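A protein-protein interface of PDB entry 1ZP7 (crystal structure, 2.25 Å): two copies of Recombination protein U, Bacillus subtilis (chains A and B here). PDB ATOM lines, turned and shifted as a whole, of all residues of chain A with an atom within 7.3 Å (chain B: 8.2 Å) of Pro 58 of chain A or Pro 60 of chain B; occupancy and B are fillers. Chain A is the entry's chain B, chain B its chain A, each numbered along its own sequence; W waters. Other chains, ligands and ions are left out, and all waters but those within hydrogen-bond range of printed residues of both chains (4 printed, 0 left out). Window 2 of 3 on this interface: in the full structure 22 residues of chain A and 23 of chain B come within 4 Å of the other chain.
Water W2 lies within hydrogen-bond range of O of Thr 59 of chain B (2.6 Å), O of Thr 59 of chain A (3.4 Å) and N of Val 61 of chain A (3.4 Å).
Water W3 bridges NZ of Lys 57 of chain B (2.8 Å) and ND1 of His 55 of chain A (3.4 Å).
Water W4 bridges the backbone carbonyl oxygen of His 55 of chain A (2.9 Å) and the side-chain amino group of Lys 57 of chain B (3.3 Å).
Water W1 bridges the backbone carbonyl oxygen of Thr 59 of chain A (3.0 Å) and the backbone NH of Val 61 of chain B (3.1 Å).
O of Pro 60 of chain B is in hydrogen-bond range of N of Lys 82 of chain B, 3.3 Å away.
OG of Ser 84 of chain B lies within hydrogen-bond range of O of Thr 86 of chain B (2.9 Å).
His 55 of chain A touches Thr 86 of chain B.
O of Pro 58 of chain B touches CG of Pro 58 of chain A, at 3.6 Å.
Pro 58 of chain A touches Pro 60 of chain B (CB to CA, 3.99 Å).
Val 61 of chain B touches Val 61 of chain A (CG2 to CG2, 3.6 Å).
Of the 10 printed residues of chain A, 3 touch a printed residue of chain B.
Of the 17 printed residues of chain B, 4 touch a printed residue of chain A.
Hydrophobic or aromatic side chains of chain B that line the printed part of chain A: Pro 58 and Val 61.
Among the printed residues, 4 pairs touch across the chains.
Printed residues of chain B within 4 Å of Pro 58 of chain A: Pro 58 and Pro 60.
Asp 88 of chain A touches none of the printed residues of chain B.
Printed residues of chain A within 4 Å of Pro 58 of chain B: Pro 58.
Of the printed residues of chain A, Pro 60 of chain B touches Pro 58.
Printed residues of chain A within 4 Å of Val 61 of chain B: Val 61.
Ala 79 of chain B touches none of the printed residues of chain A.
The nearest printed residue of chain B that does not touch Pro 58 of chain A is Thr 59 of chain B (4.4 Å).
The nearest printed residue of chain A that does not touch Pro 60 of chain B is Thr 59 of chain A (6.0 Å).
Pro 58 of chain A touches its own counterpart, Pro 58 of chain B.
Pro 58 of chain A touches Pro 60 of chain B, but with the chains exchanged Pro 60 of chain A does not touch Pro 58 of chain B (4.2 Å).
Val 61 of chain A touches its own counterpart, Val 61 of chain B.
Positions printed for both chains: 56, 57, 58, 59, 60, 61, 84, 86 and 88.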
ATOM      1  N   HIS A  55     -20.192 -28.616  38.514  1.00  0.00           N
ATOM      2  CA  HIS A  55     -19.983 -28.915  37.096  1.00  0.00           C
ATOM      3  C   HIS A  55     -18.559 -28.619  36.630  1.00  0.00           C
ATOM      4  O   HIS A  55     -17.902 -27.703  37.135  1.00  0.00           O
ATOM      5  CB  HIS A  55     -20.957 -28.115  36.207  1.00  0.00           C
ATOM      6  CG  HIS A  55     -22.395 -28.413  36.480  1.00  0.00           C
ATOM      7  ND1 HIS A  55     -23.130 -27.726  37.425  1.00  0.00           N
ATOM      8  CD2 HIS A  55     -23.226 -29.343  35.959  1.00  0.00           C
ATOM      9  CE1 HIS A  55     -24.354 -28.221  37.476  1.00  0.00           C
ATOM     10  NE2 HIS A  55     -24.436 -29.210  36.602  1.00  0.00           N
ATOM     11  N   LYS A  56     -18.099 -29.401  35.659  1.00  0.00           N
ATOM     12  CA  LYS A  56     -16.861 -29.112  34.979  1.00  0.00           C
ATOM     13  C   LYS A  56     -17.152 -27.984  33.994  1.00  0.00           C
ATOM     14  O   LYS A  56     -18.136 -28.028  33.274  1.00  0.00           O
ATOM     15  CB  LYS A  56     -16.294 -30.349  34.255  1.00  0.00           C
ATOM     16  CG  LYS A  56     -15.007 -30.036  33.454  1.00  0.00           C
ATOM     17  CD  LYS A  56     -14.341 -31.279  32.885  1.00  0.00           C
ATOM     18  CE  LYS A  56     -12.983 -30.961  32.253  1.00  0.00           C
ATOM     19  NZ  LYS A  56     -13.078 -30.044  31.057  1.00  0.00           N
ATOM     20  N   LYS A  57     -16.302 -26.967  33.987  1.00  0.00           N
ATOM     21  CA  LYS A  57     -16.396 -25.911  32.993  1.00  0.00           C
ATOM     22  C   LYS A  57     -16.060 -26.466  31.610  1.00  0.00           C
ATOM     23  O   LYS A  57     -15.216 -27.355  31.491  1.00  0.00           O
ATOM     24  CB  LYS A  57     -15.457 -24.748  33.346  1.00  0.00           C
ATOM     25  CG  LYS A  57     -15.987 -23.854  34.448  1.00  0.00           C
ATOM     26  CD  LYS A  57     -14.870 -23.155  35.198  1.00  0.00           C
ATOM     27  CE  LYS A  57     -15.384 -22.511  36.481  1.00  0.00           C
ATOM     28  NZ  LYS A  57     -15.336 -21.023  36.491  1.00  0.00           N
ATOM     29  N   PRO A  58     -16.727 -25.949  30.560  1.00  0.00           N
ATOM     30  CA  PRO A  58     -16.282 -26.244  29.198  1.00  0.00           C
ATOM     31  C   PRO A  58     -14.846 -25.787  28.987  1.00  0.00           C
ATOM     32  O   PRO A  58     -14.416 -24.791  29.577  1.00  0.00           O
ATOM     33  CB  PRO A  58     -17.218 -25.395  28.328  1.00  0.00           C
ATOM     34  CG  PRO A  58     -18.425 -25.195  29.152  1.00  0.00           C
ATOM     35  CD  PRO A  58     -17.925 -25.088  30.570  1.00  0.00           C
ATOM     36  N   THR A  59     -14.101 -26.513  28.158  1.00  0.00           N
ATOM     37  CA  THR A  59     -12.757 -26.053  27.795  1.00  0.00           C
ATOM     38  C   THR A  59     -12.896 -24.887  26.803  1.00  0.00           C
ATOM     39  O   THR A  59     -13.729 -24.952  25.894  1.00  0.00           O
ATOM     40  CB  THR A  59     -11.830 -27.194  27.247  1.00  0.00           C
ATOM     41  OG1 THR A  59     -11.633 -27.048  25.832  1.00  0.00           O
ATOM     42  CG2 THR A  59     -12.391 -28.580  27.571  1.00  0.00           C
ATOM     43  N   PRO A  60     -12.101 -23.812  26.994  1.00  0.00           N
ATOM     44  CA  PRO A  60     -12.132 -22.679  26.067  1.00  0.00           C
ATOM     45  C   PRO A  60     -11.609 -23.063  24.678  1.00  0.00           C
ATOM     46  O   PRO A  60     -10.634 -23.809  24.551  1.00  0.00           O
ATOM     47  CB  PRO A  60     -11.193 -21.646  26.708  1.00  0.00           C
ATOM     48  CG  PRO A  60     -10.846 -22.167  28.047  1.00  0.00           C
ATOM     49  CD  PRO A  60     -11.112 -23.627  28.071  1.00  0.00           C
ATOM     50  N   VAL A  61     -12.278 -22.544  23.656  1.00  0.00           N
ATOM     51  CA  VAL A  61     -11.955 -22.804  22.265  1.00  0.00           C
ATOM     52  C   VAL A  61     -11.970 -21.471  21.525  1.00  0.00           C
ATOM     53  O   VAL A  61     -12.955 -20.729  21.597  1.00  0.00           O
ATOM     54  CB  VAL A  61     -12.993 -23.770  21.638  1.00  0.00           C
ATOM     55  CG1 VAL A  61     -12.899 -23.779  20.116  1.00  0.00           C
ATOM     56  CG2 VAL A  61     -12.826 -25.171  22.197  1.00  0.00           C
ATOM     57  N   SER A  84      -7.420 -21.849  30.034  1.00  0.00           N
ATOM     58  CA  SER A  84      -8.134 -20.892  30.879  1.00  0.00           C
ATOM     59  C   SER A  84      -7.278 -20.323  32.010  1.00  0.00           C
ATOM     60  O   SER A  84      -6.252 -20.901  32.390  1.00  0.00           O
ATOM     61  CB  SER A  84      -9.409 -21.519  31.456  1.00  0.00           C
ATOM     62  OG  SER A  84      -9.109 -22.581  32.353  1.00  0.00           O
ATOM     63  N   THR A  86      -8.406 -20.242  34.863  1.00  0.00           N
ATOM     64  CA  THR A  86      -9.222 -20.752  35.951  1.00  0.00           C
ATOM     65  C   THR A  86      -9.101 -22.283  36.061  1.00  0.00           C
ATOM     66  O   THR A  86      -8.671 -22.932  35.112  1.00  0.00           O
ATOM     67  CB  THR A  86     -10.692 -20.245  35.759  1.00  0.00           C
ATOM     68  OG1 THR A  86     -11.161 -19.645  36.961  1.00  0.00           O
ATOM     69  CG2 THR A  86     -11.652 -21.330  35.306  1.00  0.00           C
ATOM     70  N   ASP A  88     -10.891 -26.147  36.476  1.00  0.00           N
ATOM     71  CA  ASP A  88     -11.994 -26.764  35.718  1.00  0.00           C
ATOM     72  C   ASP A  88     -13.319 -27.072  36.430  1.00  0.00           C
ATOM     73  O   ASP A  88     -14.334 -27.252  35.761  1.00  0.00           O
ATOM     74  CB  ASP A  88     -11.497 -28.022  34.999  1.00  0.00           C
ATOM     75  CG  ASP A  88     -10.712 -27.698  33.748  1.00  0.00           C
ATOM     76  OD1 ASP A  88     -10.749 -26.524  33.302  1.00  0.00           O
ATOM     77  OD2 ASP A  88     -10.055 -28.616  33.209  1.00  0.00           O
ATOM     78  N   LYS B  56     -17.349 -15.539  33.489  1.00  0.00           N
ATOM     79  CA  LYS B  56     -18.265 -16.137  32.528  1.00  0.00           C
ATOM     80  C   LYS B  56     -17.740 -17.505  32.081  1.00  0.00           C
ATOM     81  O   LYS B  56     -16.572 -17.635  31.710  1.00  0.00           O
ATOM     82  CB  LYS B  56     -18.467 -15.257  31.297  1.00  0.00           C
ATOM     83  CG  LYS B  56     -19.745 -15.603  30.539  1.00  0.00           C
ATOM     84  CD  LYS B  56     -19.986 -14.637  29.390  1.00  0.00           C
ATOM     85  CE  LYS B  56     -20.000 -15.353  28.062  1.00  0.00           C
ATOM     86  NZ  LYS B  56     -21.330 -15.974  27.792  1.00  0.00           N
ATOM     87  N   LYS B  57     -18.614 -18.505  32.100  1.00  0.00           N
ATOM     88  CA  LYS B  57     -18.282 -19.811  31.561  1.00  0.00           C
ATOM     89  C   LYS B  57     -18.206 -19.733  30.028  1.00  0.00           C
ATOM     90  O   LYS B  57     -19.115 -19.168  29.381  1.00  0.00           O
ATOM     91  CB  LYS B  57     -19.320 -20.847  31.985  1.00  0.00           C
ATOM     92  CG  LYS B  57     -19.336 -21.161  33.468  1.00  0.00           C
ATOM     93  CD  LYS B  57     -20.481 -22.111  33.817  1.00  0.00           C
ATOM     94  CE  LYS B  57     -20.406 -22.536  35.272  1.00  0.00           C
ATOM     95  NZ  LYS B  57     -21.320 -23.676  35.728  1.00  0.00           N
ATOM     96  N   PRO B  58     -17.126 -20.306  29.441  1.00  0.00           N
ATOM     97  CA  PRO B  58     -16.981 -20.419  27.984  1.00  0.00           C
ATOM     98  C   PRO B  58     -18.185 -21.095  27.331  1.00  0.00           C
ATOM     99  O   PRO B  58     -18.884 -21.875  27.977  1.00  0.00           O
ATOM    100  CB  PRO B  58     -15.748 -21.314  27.821  1.00  0.00           C
ATOM    101  CG  PRO B  58     -14.964 -21.092  29.035  1.00  0.00           C
ATOM    102  CD  PRO B  58     -15.968 -20.892  30.142  1.00  0.00           C
ATOM    103  N   THR B  59     -18.425 -20.789  26.063  1.00  0.00           N
ATOM    104  CA  THR B  59     -19.488 -21.462  25.304  1.00  0.00           C
ATOM    105  C   THR B  59     -19.119 -22.936  25.111  1.00  0.00           C
ATOM    106  O   THR B  59     -18.020 -23.236  24.633  1.00  0.00           O
ATOM    107  CB  THR B  59     -19.711 -20.794  23.931  1.00  0.00           C
ATOM    108  OG1 THR B  59     -19.784 -19.375  24.104  1.00  0.00           O
ATOM    109  CG2 THR B  59     -21.002 -21.300  23.272  1.00  0.00           C
ATOM    110  N   PRO B  60     -20.017 -23.859  25.508  1.00  0.00           N
ATOM    111  CA  PRO B  60     -19.734 -25.269  25.233  1.00  0.00           C
ATOM    112  C   PRO B  60     -19.773 -25.560  23.728  1.00  0.00           C
ATOM    113  O   PRO B  60     -20.668 -25.085  23.021  1.00  0.00           O
ATOM    114  CB  PRO B  60     -20.855 -26.012  25.971  1.00  0.00           C
ATOM    115  CG  PRO B  60     -21.940 -25.023  26.125  1.00  0.00           C
ATOM    116  CD  PRO B  60     -21.298 -23.673  26.214  1.00  0.00           C
ATOM    117  N   VAL B  61     -18.777 -26.305  23.254  1.00  0.00           N
ATOM    118  CA  VAL B  61     -18.708 -26.734  21.855  1.00  0.00           C
ATOM    119  C   VAL B  61     -18.640 -28.270  21.780  1.00  0.00           C
ATOM    120  O   VAL B  61     -19.097 -28.953  22.703  1.00  0.00           O
ATOM    121  CB  VAL B  61     -17.533 -26.056  21.088  1.00  0.00           C
ATOM    122  CG1 VAL B  61     -17.696 -24.534  21.069  1.00  0.00           C
ATOM    123  CG2 VAL B  61     -16.184 -26.451  21.686  1.00  0.00           C
ATOM    124  N   GLN B  62     -18.089 -28.813  20.689  1.00  0.00           N
ATOM    125  CA  GLN B  62     -17.950 -30.273  20.554  1.00  0.00           C
ATOM    126  C   GLN B  62     -16.733 -30.776  19.757  1.00  0.00           C
ATOM    127  O   GLN B  62     -15.793 -30.031  19.463  1.00  0.00           O
ATOM    128  CB  GLN B  62     -19.236 -30.889  19.995  1.00  0.00           C
ATOM    129  CG  GLN B  62     -19.687 -32.121  20.778  1.00  0.00           C
ATOM    130  CD  GLN B  62     -20.693 -32.979  20.025  1.00  0.00           C
ATOM    131  OE1 GLN B  62     -20.690 -34.204  20.155  1.00  0.00           O
ATOM    132  NE2 GLN B  62     -21.560 -32.340  19.239  1.00  0.00           N
ATOM    133  N   ALA B  79     -16.836 -29.727  15.205  1.00  0.00           N
ATOM    134  CA  ALA B  79     -17.085 -29.007  16.442  1.00  0.00           C
ATOM    135  C   ALA B  79     -18.336 -28.161  16.270  1.00  0.00           C
ATOM    136  O   ALA B  79     -18.370 -27.242  15.449  1.00  0.00           O
ATOM    137  CB  ALA B  79     -15.890 -28.138  16.812  1.00  0.00           C
ATOM    138  N   TYR B  80     -19.368 -28.503  17.034  1.00  0.00           N
ATOM    139  CA  TYR B  80     -20.655 -27.826  16.964  1.00  0.00           C
ATOM    140  C   TYR B  80     -20.953 -27.128  18.290  1.00  0.00           C
ATOM    141  O   TYR B  80     -20.366 -27.467  19.319  1.00  0.00           O
ATOM    142  CB  TYR B  80     -21.759 -28.847  16.650  1.00  0.00           C
ATOM    143  CG  TYR B  80     -21.685 -29.470  15.260  1.00  0.00           C
ATOM    144  CD1 TYR B  80     -20.503 -30.057  14.790  1.00  0.00           C
ATOM    145  CD2 TYR B  80     -22.814 -29.500  14.425  1.00  0.00           C
ATOM    146  CE1 TYR B  80     -20.433 -30.633  13.524  1.00  0.00           C
ATOM    147  CE2 TYR B  80     -22.757 -30.082  13.154  1.00  0.00           C
ATOM    148  CZ  TYR B  80     -21.561 -30.646  12.713  1.00  0.00           C
ATOM    149  OH  TYR B  80     -21.483 -31.224  11.466  1.00  0.00           O
ATOM    150  N   PHE B  81     -21.864 -26.155  18.263  1.00  0.00           N
ATOM    151  CA  PHE B  81     -22.350 -25.533  19.493  1.00  0.00           C
ATOM    152  C   PHE B  81     -23.332 -26.448  20.221  1.00  0.00           C
ATOM    153  O   PHE B  81     -24.331 -26.892  19.645  1.00  0.00           O
ATOM    154  CB  PHE B  81     -22.997 -24.168  19.218  1.00  0.00           C
ATOM    155  CG  PHE B  81     -22.030 -23.122  18.733  1.00  0.00           C
ATOM    156  CD1 PHE B  81     -22.185 -22.544  17.479  1.00  0.00           C
ATOM    157  CD2 PHE B  81     -20.957 -22.721  19.527  1.00  0.00           C
ATOM    158  CE1 PHE B  81     -21.287 -21.575  17.018  1.00  0.00           C
ATOM    159  CE2 PHE B  81     -20.053 -21.757  19.079  1.00  0.00           C
ATOM    160  CZ  PHE B  81     -20.222 -21.181  17.819  1.00  0.00           C
ATOM    161  N   LYS B  82     -23.009 -26.760  21.474  1.00  0.00           N
ATOM    162  CA  LYS B  82     -23.976 -27.313  22.413  1.00  0.00           C
ATOM    163  C   LYS B  82     -24.542 -26.120  23.173  1.00  0.00           C
ATOM    164  O   LYS B  82     -23.999 -25.010  23.085  1.00  0.00           O
ATOM    165  CB  LYS B  82     -23.311 -28.308  23.365  1.00  0.00           C
ATOM    166  N   GLN B  83     -25.615 -26.334  23.926  1.00  0.00           N
ATOM    167  CA  GLN B  83     -26.311 -25.211  24.539  1.00  0.00           C
ATOM    168  C   GLN B  83     -25.773 -24.775  25.911  1.00  0.00           C
ATOM    169  O   GLN B  83     -25.622 -23.569  26.162  1.00  0.00           O
ATOM    170  CB  GLN B  83     -27.809 -25.489  24.616  1.00  0.00           C
ATOM    171  CG  GLN B  83     -28.645 -24.230  24.751  1.00  0.00           C
ATOM    172  CD  GLN B  83     -30.119 -24.534  24.857  1.00  0.00           C
ATOM    173  OE1 GLN B  83     -30.558 -25.272  25.750  1.00  0.00           O
ATOM    174  NE2 GLN B  83     -30.899 -23.972  23.942  1.00  0.00           N
ATOM    175  N   SER B  84     -25.478 -25.763  26.763  1.00  0.00           N
ATOM    176  CA  SER B  84     -25.213 -25.604  28.211  1.00  0.00           C
ATOM    177  C   SER B  84     -26.445 -26.174  28.898  1.00  0.00           C
ATOM    178  O   SER B  84     -27.493 -26.356  28.278  1.00  0.00           O
ATOM    179  CB  SER B  84     -24.629 -24.231  28.582  1.00  0.00           C
ATOM    180  OG  SER B  84     -24.529 -24.083  29.995  1.00  0.00           O
ATOM    181  N   SER B  85     -26.309 -26.467  30.184  1.00  0.00           N
ATOM    182  CA  SER B  85     -27.425 -26.968  30.984  1.00  0.00           C
ATOM    183  C   SER B  85     -27.382 -26.059  32.211  1.00  0.00           C
ATOM    184  O   SER B  85     -28.087 -26.282  33.195  1.00  0.00           O
ATOM    185  CB  SER B  85     -27.345 -28.430  31.418  1.00  0.00           C
ATOM    186  OG  SER B  85     -26.192 -28.637  32.223  1.00  0.00           O
ATOM    187  N   THR B  86     -26.550 -25.026  32.117  1.00  0.00           N
ATOM    188  CA  THR B  86     -26.131 -24.206  33.247  1.00  0.00           C
ATOM    189  C   THR B  86     -26.217 -22.715  32.852  1.00  0.00           C
ATOM    190  O   THR B  86     -26.191 -22.392  31.668  1.00  0.00           O
ATOM    191  CB  THR B  86     -24.663 -24.640  33.660  1.00  0.00           C
ATOM    192  OG1 THR B  86     -24.693 -25.555  34.774  1.00  0.00           O
ATOM    193  CG2 THR B  86     -23.793 -23.482  33.979  1.00  0.00           C
ATOM    194  N   THR B  87     -26.332 -21.824  33.838  1.00  0.00           N
ATOM    195  CA  THR B  87     -26.184 -20.363  33.621  1.00  0.00           C
ATOM    196  C   THR B  87     -24.726 -20.003  33.341  1.00  0.00           C
ATOM    197  O   THR B  87     -23.832 -20.734  33.752  1.00  0.00           O
ATOM    198  CB  THR B  87     -26.658 -19.566  34.847  1.00  0.00           C
ATOM    199  OG1 THR B  87     -26.006 -20.078  36.015  1.00  0.00           O
ATOM    200  CG2 THR B  87     -28.167 -19.699  35.020  1.00  0.00           C
ATOM    201  N   ASP B  88     -24.482 -18.881  32.665  1.00  0.00           N
ATOM    202  CA  ASP B  88     -23.118 -18.495  32.284  1.00  0.00           C
ATOM    203  C   ASP B  88     -22.159 -17.948  33.363  1.00  0.00           C
ATOM    204  O   ASP B  88     -20.940 -18.034  33.180  1.00  0.00           O
ATOM    205  CB  ASP B  88     -23.131 -17.515  31.115  1.00  0.00           C
ATOM    206  CG  ASP B  88     -23.441 -18.195  29.801  1.00  0.00           C
ATOM    207  OD1 ASP B  88     -23.582 -19.437  29.777  1.00  0.00           O
ATOM    208  OD2 ASP B  88     -23.560 -17.490  28.788  1.00  0.00           O
HETATM  209  O   HOH W   1     -16.293 -26.339  25.069  1.00  0.00           O
HETATM  210  O   HOH W   2     -15.582 -22.419  24.617  1.00  0.00           O
HETATM  211  O   HOH W   3     -21.224 -24.983  38.170  1.00  0.00           O
HETATM  212  O   HOH W   4     -18.349 -24.945  36.451  1.00  0.00           O
